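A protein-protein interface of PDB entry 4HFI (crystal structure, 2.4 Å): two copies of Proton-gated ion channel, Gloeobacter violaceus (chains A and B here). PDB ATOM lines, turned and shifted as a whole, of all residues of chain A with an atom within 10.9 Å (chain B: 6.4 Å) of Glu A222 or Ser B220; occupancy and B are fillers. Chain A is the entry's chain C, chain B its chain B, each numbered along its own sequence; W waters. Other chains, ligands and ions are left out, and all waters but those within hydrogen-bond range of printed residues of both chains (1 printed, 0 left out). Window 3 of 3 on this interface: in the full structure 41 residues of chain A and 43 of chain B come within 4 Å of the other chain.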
ATOM      1  N   ALA A 215      -2.849   4.013  32.087  1.00  0.00           N
ATOM      2  CA  ALA A 215      -2.300   2.763  31.561  1.00  0.00           C
ATOM      3  C   ALA A 215      -3.137   1.563  32.024  1.00  0.00           C
ATOM      4  O   ALA A 215      -3.062   0.498  31.411  1.00  0.00           O
ATOM      5  CB  ALA A 215      -0.850   2.600  32.010  1.00  0.00           C
ATOM      6  N   SER A 218      -5.735   0.728  29.317  1.00  0.00           N
ATOM      7  CA  SER A 218      -5.079   0.483  28.039  1.00  0.00           C
ATOM      8  C   SER A 218      -4.425  -0.893  27.999  1.00  0.00           C
ATOM      9  O   SER A 218      -3.786  -1.310  28.968  1.00  0.00           O
ATOM     10  CB  SER A 218      -4.042   1.564  27.752  1.00  0.00           C
ATOM     11  OG  SER A 218      -3.100   1.163  26.768  1.00  0.00           O
ATOM     12  N   THR A 219      -4.580  -1.573  26.855  1.00  0.00           N
ATOM     13  CA  THR A 219      -4.018  -2.898  26.570  1.00  0.00           C
ATOM     14  C   THR A 219      -2.739  -2.770  25.726  1.00  0.00           C
ATOM     15  O   THR A 219      -1.993  -3.742  25.584  1.00  0.00           O
ATOM     16  CB  THR A 219      -5.081  -3.816  25.928  1.00  0.00           C
ATOM     17  OG1 THR A 219      -5.748  -3.110  24.874  1.00  0.00           O
ATOM     18  CG2 THR A 219      -6.103  -4.320  26.940  1.00  0.00           C
ATOM     19  N   SER A 220      -2.479  -1.559  25.194  1.00  0.00           N
ATOM     20  CA  SER A 220      -1.306  -1.242  24.389  1.00  0.00           C
ATOM     21  C   SER A 220      -0.069  -1.105  25.273  1.00  0.00           C
ATOM     22  O   SER A 220       0.104  -0.078  25.929  1.00  0.00           O
ATOM     23  CB  SER A 220      -1.544   0.026  23.574  1.00  0.00           C
ATOM     24  OG  SER A 220      -0.383   0.403  22.851  1.00  0.00           O
ATOM     25  N   TYR A 221       0.789  -2.141  25.289  1.00  0.00           N
ATOM     26  CA  TYR A 221       2.033  -2.182  26.062  1.00  0.00           C
ATOM     27  C   TYR A 221       2.988  -1.032  25.715  1.00  0.00           C
ATOM     28  O   TYR A 221       3.537  -0.401  26.620  1.00  0.00           O
ATOM     29  CB  TYR A 221       2.739  -3.534  25.859  1.00  0.00           C
ATOM     30  CG  TYR A 221       4.040  -3.696  26.620  1.00  0.00           C
ATOM     31  CD1 TYR A 221       4.091  -3.513  28.001  1.00  0.00           C
ATOM     32  CD2 TYR A 221       5.206  -4.091  25.971  1.00  0.00           C
ATOM     33  CE1 TYR A 221       5.270  -3.715  28.714  1.00  0.00           C
ATOM     34  CE2 TYR A 221       6.394  -4.283  26.674  1.00  0.00           C
ATOM     35  CZ  TYR A 221       6.424  -4.082  28.045  1.00  0.00           C
ATOM     36  OH  TYR A 221       7.591  -4.257  28.747  1.00  0.00           O
ATOM     37  N   GLU A 222       3.174  -0.768  24.411  1.00  0.00           N
ATOM     38  CA  GLU A 222       4.056   0.271  23.877  1.00  0.00           C
ATOM     39  C   GLU A 222       3.630   1.681  24.355  1.00  0.00           C
ATOM     40  O   GLU A 222       4.484   2.515  24.658  1.00  0.00           O
ATOM     41  CB  GLU A 222       4.127   0.189  22.332  1.00  0.00           C
ATOM     42  CG  GLU A 222       4.488  -1.184  21.746  1.00  0.00           C
ATOM     43  CD  GLU A 222       3.475  -2.325  21.821  1.00  0.00           C
ATOM     44  OE1 GLU A 222       2.250  -2.059  21.816  1.00  0.00           O
ATOM     45  OE2 GLU A 222       3.916  -3.497  21.885  1.00  0.00           O
ATOM     46  N   ALA A 223       2.312   1.933  24.427  1.00  0.00           N
ATOM     47  CA  ALA A 223       1.738   3.199  24.885  1.00  0.00           C
ATOM     48  C   ALA A 223       1.820   3.292  26.411  1.00  0.00           C
ATOM     49  O   ALA A 223       2.070   4.374  26.946  1.00  0.00           O
ATOM     50  CB  ALA A 223       0.291   3.314  24.426  1.00  0.00           C
ATOM     51  N   ASN A 224       1.623   2.149  27.106  1.00  0.00           N
ATOM     52  CA  ASN A 224       1.703   2.036  28.563  1.00  0.00           C
ATOM     53  C   ASN A 224       3.115   2.323  29.058  1.00  0.00           C
ATOM     54  O   ASN A 224       3.274   3.073  30.016  1.00  0.00           O
ATOM     55  CB  ASN A 224       1.233   0.656  29.023  1.00  0.00           C
ATOM     56  CG  ASN A 224      -0.257   0.457  28.927  1.00  0.00           C
ATOM     57  OD1 ASN A 224      -1.016   1.381  28.613  1.00  0.00           O
ATOM     58  ND2 ASN A 224      -0.705  -0.763  29.176  1.00  0.00           N
ATOM     59  N   VAL A 225       4.136   1.764  28.372  1.00  0.00           N
ATOM     60  CA  VAL A 225       5.556   1.974  28.675  1.00  0.00           C
ATOM     61  C   VAL A 225       5.853   3.474  28.538  1.00  0.00           C
ATOM     62  O   VAL A 225       6.449   4.059  29.435  1.00  0.00           O
ATOM     63  CB  VAL A 225       6.455   1.060  27.787  1.00  0.00           C
ATOM     64  CG1 VAL A 225       7.886   1.578  27.681  1.00  0.00           C
ATOM     65  CG2 VAL A 225       6.450  -0.367  28.309  1.00  0.00           C
ATOM     66  N   THR A 226       5.348   4.101  27.459  1.00  0.00           N
ATOM     67  CA  THR A 226       5.494   5.533  27.195  1.00  0.00           C
ATOM     68  C   THR A 226       4.830   6.364  28.299  1.00  0.00           C
ATOM     69  O   THR A 226       5.441   7.315  28.772  1.00  0.00           O
ATOM     70  CB  THR A 226       5.009   5.871  25.775  1.00  0.00           C
ATOM     71  OG1 THR A 226       5.770   5.094  24.849  1.00  0.00           O
ATOM     72  CG2 THR A 226       5.163   7.352  25.433  1.00  0.00           C
ATOM     73  N   LEU A 227       3.615   5.983  28.731  1.00  0.00           N
ATOM     74  CA  LEU A 227       2.876   6.680  29.789  1.00  0.00           C
ATOM     75  C   LEU A 227       3.601   6.667  31.139  1.00  0.00           C
ATOM     76  O   LEU A 227       3.752   7.721  31.751  1.00  0.00           O
ATOM     77  CB  LEU A 227       1.463   6.082  29.971  1.00  0.00           C
ATOM     78  CG  LEU A 227       0.361   6.565  29.038  1.00  0.00           C
ATOM     79  CD1 LEU A 227      -0.789   5.566  29.000  1.00  0.00           C
ATOM     80  CD2 LEU A 227      -0.159   7.941  29.451  1.00  0.00           C
ATOM     81  N   VAL A 228       4.014   5.477  31.615  1.00  0.00           N
ATOM     82  CA  VAL A 228       4.646   5.302  32.927  1.00  0.00           C
ATOM     83  C   VAL A 228       6.087   5.828  32.988  1.00  0.00           C
ATOM     84  O   VAL A 228       6.444   6.501  33.955  1.00  0.00           O
ATOM     85  CB  VAL A 228       4.484   3.859  33.500  1.00  0.00           C
ATOM     86  CG1 VAL A 228       4.859   3.805  34.978  1.00  0.00           C
ATOM     87  CG2 VAL A 228       3.060   3.343  33.309  1.00  0.00           C
ATOM     88  N   VAL A 229       6.898   5.549  31.954  1.00  0.00           N
ATOM     89  CA  VAL A 229       8.297   5.978  31.907  1.00  0.00           C
ATOM     90  C   VAL A 229       8.447   7.500  31.745  1.00  0.00           C
ATOM     91  O   VAL A 229       9.249   8.100  32.459  1.00  0.00           O
ATOM     92  CB  VAL A 229       9.155   5.141  30.915  1.00  0.00           C
ATOM     93  CG1 VAL A 229      10.600   5.612  30.902  1.00  0.00           C
ATOM     94  CG2 VAL A 229       9.101   3.651  31.265  1.00  0.00           C
ATOM     95  N   SER A 230       7.651   8.122  30.856  1.00  0.00           N
ATOM     96  CA  SER A 230       7.700   9.576  30.627  1.00  0.00           C
ATOM     97  C   SER A 230       7.292  10.373  31.860  1.00  0.00           C
ATOM     98  O   SER A 230       7.944  11.370  32.176  1.00  0.00           O
ATOM     99  CB  SER A 230       6.824   9.972  29.445  1.00  0.00           C
ATOM    100  OG  SER A 230       7.278   9.385  28.240  1.00  0.00           O
ATOM    101  N   VAL A 270       4.920  -0.118  36.589  1.00  0.00           N
ATOM    102  CA  VAL A 270       5.749  -0.740  35.542  1.00  0.00           C
ATOM    103  C   VAL A 270       5.580  -2.271  35.630  1.00  0.00           C
ATOM    104  O   VAL A 270       5.393  -2.913  34.594  1.00  0.00           O
ATOM    105  CB  VAL A 270       7.244  -0.300  35.613  1.00  0.00           C
ATOM    106  CG1 VAL A 270       8.116  -1.098  34.643  1.00  0.00           C
ATOM    107  CG2 VAL A 270       7.397   1.191  35.341  1.00  0.00           C
ATOM    108  N   VAL A 273       2.145  -3.201  34.226  1.00  0.00           N
ATOM    109  CA  VAL A 273       2.194  -3.042  32.767  1.00  0.00           C
ATOM    110  C   VAL A 273       2.971  -4.212  32.109  1.00  0.00           C
ATOM    111  O   VAL A 273       2.575  -4.686  31.036  1.00  0.00           O
ATOM    112  CB  VAL A 273       2.747  -1.634  32.411  1.00  0.00           C
ATOM    113  CG1 VAL A 273       3.317  -1.572  30.998  1.00  0.00           C
ATOM    114  CG2 VAL A 273       1.678  -0.565  32.610  1.00  0.00           C
ATOM    115  N   THR A 274       4.059  -4.680  32.774  1.00  0.00           N
ATOM    116  CA  THR A 274       4.896  -5.800  32.330  1.00  0.00           C
ATOM    117  C   THR A 274       4.113  -7.110  32.446  1.00  0.00           C
ATOM    118  O   THR A 274       4.074  -7.876  31.485  1.00  0.00           O
ATOM    119  CB  THR A 274       6.223  -5.832  33.118  1.00  0.00           C
ATOM    120  OG1 THR A 274       6.839  -4.542  33.065  1.00  0.00           O
ATOM    121  CG2 THR A 274       7.198  -6.901  32.604  1.00  0.00           C
ATOM    122  N   GLN A 276       0.806  -7.524  32.704  1.00  0.00           N
ATOM    123  CA  GLN A 276      -0.307  -7.434  31.755  1.00  0.00           C
ATOM    124  C   GLN A 276       0.127  -7.889  30.357  1.00  0.00           C
ATOM    125  O   GLN A 276      -0.504  -8.781  29.802  1.00  0.00           O
ATOM    126  CB  GLN A 276      -0.885  -6.008  31.723  1.00  0.00           C
ATOM    127  CG  GLN A 276      -2.060  -5.818  30.752  1.00  0.00           C
ATOM    128  CD  GLN A 276      -2.309  -4.364  30.421  1.00  0.00           C
ATOM    129  OE1 GLN A 276      -1.380  -3.569  30.209  1.00  0.00           O
ATOM    130  NE2 GLN A 276      -3.578  -3.991  30.329  1.00  0.00           N
ATOM    131  N   HIS A 277       1.220  -7.312  29.818  1.00  0.00           N
ATOM    132  CA  HIS A 277       1.760  -7.657  28.501  1.00  0.00           C
ATOM    133  C   HIS A 277       2.181  -9.123  28.404  1.00  0.00           C
ATOM    134  O   HIS A 277       1.842  -9.783  27.424  1.00  0.00           O
ATOM    135  CB  HIS A 277       2.936  -6.748  28.144  1.00  0.00           C
ATOM    136  CG  HIS A 277       3.595  -7.079  26.838  1.00  0.00           C
ATOM    137  ND1 HIS A 277       2.938  -6.907  25.635  1.00  0.00           N
ATOM    138  CD2 HIS A 277       4.841  -7.546  26.593  1.00  0.00           C
ATOM    139  CE1 HIS A 277       3.800  -7.273  24.698  1.00  0.00           C
ATOM    140  NE2 HIS A 277       4.956  -7.670  25.230  1.00  0.00           N
ATOM    141  N   TYR A 278       2.916  -9.618  29.421  1.00  0.00           N
ATOM    142  CA  TYR A 278       3.414 -10.991  29.504  1.00  0.00           C
ATOM    143  C   TYR A 278       2.277 -12.017  29.388  1.00  0.00           C
ATOM    144  O   TYR A 278       2.406 -12.975  28.625  1.00  0.00           O
ATOM    145  CB  TYR A 278       4.217 -11.196  30.805  1.00  0.00           C
ATOM    146  CG  TYR A 278       4.993 -12.495  30.852  1.00  0.00           C
ATOM    147  CD1 TYR A 278       4.428 -13.650  31.385  1.00  0.00           C
ATOM    148  CD2 TYR A 278       6.295 -12.569  30.368  1.00  0.00           C
ATOM    149  CE1 TYR A 278       5.137 -14.849  31.429  1.00  0.00           C
ATOM    150  CE2 TYR A 278       7.016 -13.762  30.410  1.00  0.00           C
ATOM    151  CZ  TYR A 278       6.431 -14.901  30.941  1.00  0.00           C
ATOM    152  OH  TYR A 278       7.138 -16.079  30.986  1.00  0.00           O
ATOM    153  N   LYS A 280      -0.849 -11.488  28.140  1.00  0.00           N
ATOM    154  CA  LYS A 280      -1.502 -11.362  26.831  1.00  0.00           C
ATOM    155  C   LYS A 280      -0.713 -12.106  25.753  1.00  0.00           C
ATOM    156  O   LYS A 280      -1.327 -12.754  24.907  1.00  0.00           O
ATOM    157  CB  LYS A 280      -1.716  -9.892  26.434  1.00  0.00           C
ATOM    158  CG  LYS A 280      -2.524  -9.080  27.450  1.00  0.00           C
ATOM    159  CD  LYS A 280      -3.904  -8.665  26.969  1.00  0.00           C
ATOM    160  CE  LYS A 280      -4.529  -7.669  27.915  1.00  0.00           C
ATOM    161  NZ  LYS A 280      -5.847  -8.118  28.435  1.00  0.00           N
ATOM    162  N   VAL A 281       0.632 -12.052  25.807  1.00  0.00           N
ATOM    163  CA  VAL A 281       1.533 -12.751  24.879  1.00  0.00           C
ATOM    164  C   VAL A 281       1.408 -14.283  25.100  1.00  0.00           C
ATOM    165  O   VAL A 281       1.455 -15.055  24.141  1.00  0.00           O
ATOM    166  CB  VAL A 281       2.989 -12.214  25.029  1.00  0.00           C
ATOM    167  CG1 VAL A 281       4.004 -13.086  24.294  1.00  0.00           C
ATOM    168  CG2 VAL A 281       3.087 -10.772  24.544  1.00  0.00           C
ATOM    169  N   ALA B 215      12.514  -5.218  30.372  1.00  0.00           N
ATOM    170  CA  ALA B 215      12.693  -5.501  28.948  1.00  0.00           C
ATOM    171  C   ALA B 215      13.037  -6.979  28.731  1.00  0.00           C
ATOM    172  O   ALA B 215      12.877  -7.482  27.617  1.00  0.00           O
ATOM    173  CB  ALA B 215      13.791  -4.614  28.375  1.00  0.00           C
ATOM    174  N   SER B 218       9.813  -8.935  27.969  1.00  0.00           N
ATOM    175  CA  SER B 218       9.127  -8.359  26.820  1.00  0.00           C
ATOM    176  C   SER B 218       9.800  -8.742  25.512  1.00  0.00           C
ATOM    177  O   SER B 218      11.032  -8.718  25.406  1.00  0.00           O
ATOM    178  CB  SER B 218       9.055  -6.840  26.954  1.00  0.00           C
ATOM    179  OG  SER B 218       8.790  -6.205  25.713  1.00  0.00           O
ATOM    180  N   THR B 219       8.970  -9.070  24.509  1.00  0.00           N
ATOM    181  CA  THR B 219       9.378  -9.434  23.148  1.00  0.00           C
ATOM    182  C   THR B 219       9.226  -8.230  22.202  1.00  0.00           C
ATOM    183  O   THR B 219       9.732  -8.261  21.077  1.00  0.00           O
ATOM    184  CB  THR B 219       8.613 -10.685  22.665  1.00  0.00           C
ATOM    185  OG1 THR B 219       7.214 -10.536  22.950  1.00  0.00           O
ATOM    186  CG2 THR B 219       9.133 -11.966  23.312  1.00  0.00           C
ATOM    187  N   SER B 220       8.547  -7.166  22.673  1.00  0.00           N
ATOM    188  CA  SER B 220       8.319  -5.928  21.932  1.00  0.00           C
ATOM    189  C   SER B 220       9.603  -5.086  21.893  1.00  0.00           C
ATOM    190  O   SER B 220       9.940  -4.435  22.877  1.00  0.00           O
ATOM    191  CB  SER B 220       7.167  -5.142  22.553  1.00  0.00           C
ATOM    192  OG  SER B 220       6.982  -3.892  21.912  1.00  0.00           O
ATOM    193  N   TYR B 221      10.310  -5.104  20.753  1.00  0.00           N
ATOM    194  CA  TYR B 221      11.549  -4.352  20.529  1.00  0.00           C
ATOM    195  C   TYR B 221      11.374  -2.844  20.714  1.00  0.00           C
ATOM    196  O   TYR B 221      12.202  -2.215  21.373  1.00  0.00           O
ATOM    197  CB  TYR B 221      12.116  -4.658  19.132  1.00  0.00           C
ATOM    198  CG  TYR B 221      13.407  -3.933  18.796  1.00  0.00           C
ATOM    199  CD1 TYR B 221      14.530  -4.048  19.611  1.00  0.00           C
ATOM    200  CD2 TYR B 221      13.526  -3.189  17.625  1.00  0.00           C
ATOM    201  CE1 TYR B 221      15.736  -3.436  19.277  1.00  0.00           C
ATOM    202  CE2 TYR B 221      14.724  -2.559  17.289  1.00  0.00           C
ATOM    203  CZ  TYR B 221      15.823  -2.676  18.121  1.00  0.00           C
ATOM    204  OH  TYR B 221      17.002  -2.050  17.796  1.00  0.00           O
ATOM    205  N   GLU B 222      10.312  -2.266  20.130  1.00  0.00           N
ATOM    206  CA  GLU B 222      10.029  -0.834  20.220  1.00  0.00           C
ATOM    207  C   GLU B 222       9.757  -0.348  21.656  1.00  0.00           C
ATOM    208  O   GLU B 222      10.153   0.767  22.003  1.00  0.00           O
ATOM    209  CB  GLU B 222       8.985  -0.347  19.183  1.00  0.00           C
ATOM    210  CG  GLU B 222       7.971  -1.377  18.683  1.00  0.00           C
ATOM    211  CD  GLU B 222       8.472  -2.526  17.817  1.00  0.00           C
ATOM    212  OE1 GLU B 222       8.138  -3.692  18.138  1.00  0.00           O
ATOM    213  OE2 GLU B 222       9.203  -2.268  16.832  1.00  0.00           O
ATOM    214  N   ALA B 223       9.136  -1.207  22.495  1.00  0.00           N
ATOM    215  CA  ALA B 223       8.872  -0.921  23.908  1.00  0.00           C
ATOM    216  C   ALA B 223      10.157  -1.102  24.721  1.00  0.00           C
ATOM    217  O   ALA B 223      10.407  -0.335  25.649  1.00  0.00           O
ATOM    218  CB  ALA B 223       7.777  -1.834  24.438  1.00  0.00           C
ATOM    219  N   ASN B 224      10.974  -2.107  24.356  1.00  0.00           N
ATOM    220  CA  ASN B 224      12.264  -2.406  24.986  1.00  0.00           C
ATOM    221  C   ASN B 224      13.251  -1.267  24.776  1.00  0.00           C
ATOM    222  O   ASN B 224      13.912  -0.860  25.729  1.00  0.00           O
ATOM    223  CB  ASN B 224      12.829  -3.724  24.455  1.00  0.00           C
ATOM    224  CG  ASN B 224      12.117  -4.945  24.973  1.00  0.00           C
ATOM    225  OD1 ASN B 224      11.233  -4.867  25.832  1.00  0.00           O
ATOM    226  ND2 ASN B 224      12.476  -6.103  24.451  1.00  0.00           N
ATOM    227  N   VAL B 225      13.315  -0.725  23.539  1.00  0.00           N
ATOM    228  CA  VAL B 225      14.161   0.413  23.169  1.00  0.00           C
ATOM    229  C   VAL B 225      13.749   1.610  24.035  1.00  0.00           C
ATOM    230  O   VAL B 225      14.612   2.244  24.641  1.00  0.00           O
ATOM    231  CB  VAL B 225      14.100   0.680  21.634  1.00  0.00           C
ATOM    232  CG1 VAL B 225      14.524   2.102  21.275  1.00  0.00           C
ATOM    233  CG2 VAL B 225      14.947  -0.329  20.878  1.00  0.00           C
ATOM    234  N   THR B 226      12.430   1.845  24.172  1.00  0.00           N
ATOM    235  CA  THR B 226      11.863   2.912  24.992  1.00  0.00           C
ATOM    236  C   THR B 226      12.233   2.729  26.470  1.00  0.00           C
ATOM    237  O   THR B 226      12.630   3.695  27.106  1.00  0.00           O
ATOM    238  CB  THR B 226      10.351   3.042  24.737  1.00  0.00           C
ATOM    239  OG1 THR B 226      10.158   3.309  23.348  1.00  0.00           O
ATOM    240  CG2 THR B 226       9.700   4.158  25.561  1.00  0.00           C
ATOM    241  N   VAL B 273      18.746  -6.509  23.948  1.00  0.00           N
ATOM    242  CA  VAL B 273      17.506  -6.081  23.291  1.00  0.00           C
ATOM    243  C   VAL B 273      17.653  -6.123  21.754  1.00  0.00           C
ATOM    244  O   VAL B 273      16.723  -6.545  21.061  1.00  0.00           O
ATOM    245  CB  VAL B 273      17.047  -4.707  23.859  1.00  0.00           C
ATOM    246  CG1 VAL B 273      16.135  -3.947  22.902  1.00  0.00           C
ATOM    247  CG2 VAL B 273      16.376  -4.882  25.217  1.00  0.00           C
ATOM    248  N   GLN B 276      18.106  -9.973  20.716  1.00  0.00           N
ATOM    249  CA  GLN B 276      16.770 -10.564  20.823  1.00  0.00           C
ATOM    250  C   GLN B 276      15.935 -10.260  19.574  1.00  0.00           C
ATOM    251  O   GLN B 276      15.433 -11.195  18.954  1.00  0.00           O
ATOM    252  CB  GLN B 276      16.059 -10.078  22.098  1.00  0.00           C
ATOM    253  CG  GLN B 276      14.639 -10.631  22.290  1.00  0.00           C
ATOM    254  CD  GLN B 276      13.820  -9.816  23.267  1.00  0.00           C
ATOM    255  OE1 GLN B 276      13.844  -8.574  23.273  1.00  0.00           O
ATOM    256  NE2 GLN B 276      13.047 -10.503  24.093  1.00  0.00           N
HETATM  257  O   HOH W   1       7.012   2.701  22.588  1.00  0.00           O
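Among the printed residues, merely in contact across the chains: Tyr A221 with Ser B218 (3.2 Å), Tyr A221 with Ala B223 (3.6 Å), Val A225 with Ala B223 (3.8 Å) and Val A225 with Thr B226 (3.8 Å).
Glu A222 touches one residue of chain B.
Ser B220 touches one residue of chain A.
No residue of chain A comes within 4 Å of Thr B219.
No residue of chain A comes within 4 Å of Asn B224.
Of the printed residues of chain B, Tyr A221 touches Ser B218 and Ala B223.
Printed residues of chain A within 4 Å of Thr B226: Val A225 (3.8 Å).
Of the printed residues of chain B, Val A225 touches Ala B223 and Thr B226.
Leu A227 touches none of the printed residues of chain B.
Val A273 touches none of the printed residues of chain B.
The nearest printed residue of chain B that does not touch Val A225 is Asn B224 (5.8 Å).
Tyr A221 touches Ser B218, but with the chains exchanged Ser A218 does not touch Tyr B221 (16.0 Å).
Tyr A221 touches Ala B223, but with the chains exchanged Ala A223 does not touch Tyr B221 (10.9 Å).
Val A225 touches Ala B223, but with the chains exchanged Ala A223 does not touch Val B225 (11.4 Å).
Val A225 touches Thr B226, but with the chains exchanged Thr A226 does not touch Val B225 (8.7 Å).
Water W1 bridges the backbone carbonyl oxygen (O) of Glu A222 (3.3 Å) and the side-chain hydroxyl (OG1) of Thr B226 (3.3 Å).
The side-chain hydroxyl (OG1) of Thr A226 is in hydrogen-bond range of the backbone carbonyl oxygen (O) of Glu A222, at 2.9 Å.
The side-chain hydroxyl of Ser B220 sits close to the backbone NH of Ala B223.
The backbone carbonyl oxygen of Ser B218 lies within hydrogen-bond range of the side-chain amide nitrogen of Gln B276.
The backbone carbonyl oxygen of Ser B220 sits close to the side-chain amide oxygen of Asn B224, at 3.3 Å.
The backbone NH of Ser B220 lies within hydrogen-bond range of the side-chain hydroxyl of Ser B218 (3.2 Å).
The side-chain hydroxyl (OG) of Ser B218 sits at hydrogen-bond distance from the side-chain amide oxygen (OD1) of Asn B224 (2.8 Å).
Printed residues of chain B that touch a printed residue of chain A: Ser B218, Ser B220, Ala B223 and Thr B226.
Among the printed residues, no Asp or Glu carboxylate lies within 4 Å of a Lys or Arg side-chain nitrogen of the other chain.
OE2 of Glu A222 sits at hydrogen-bond distance from OG of Ser B220 (3.1 Å).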
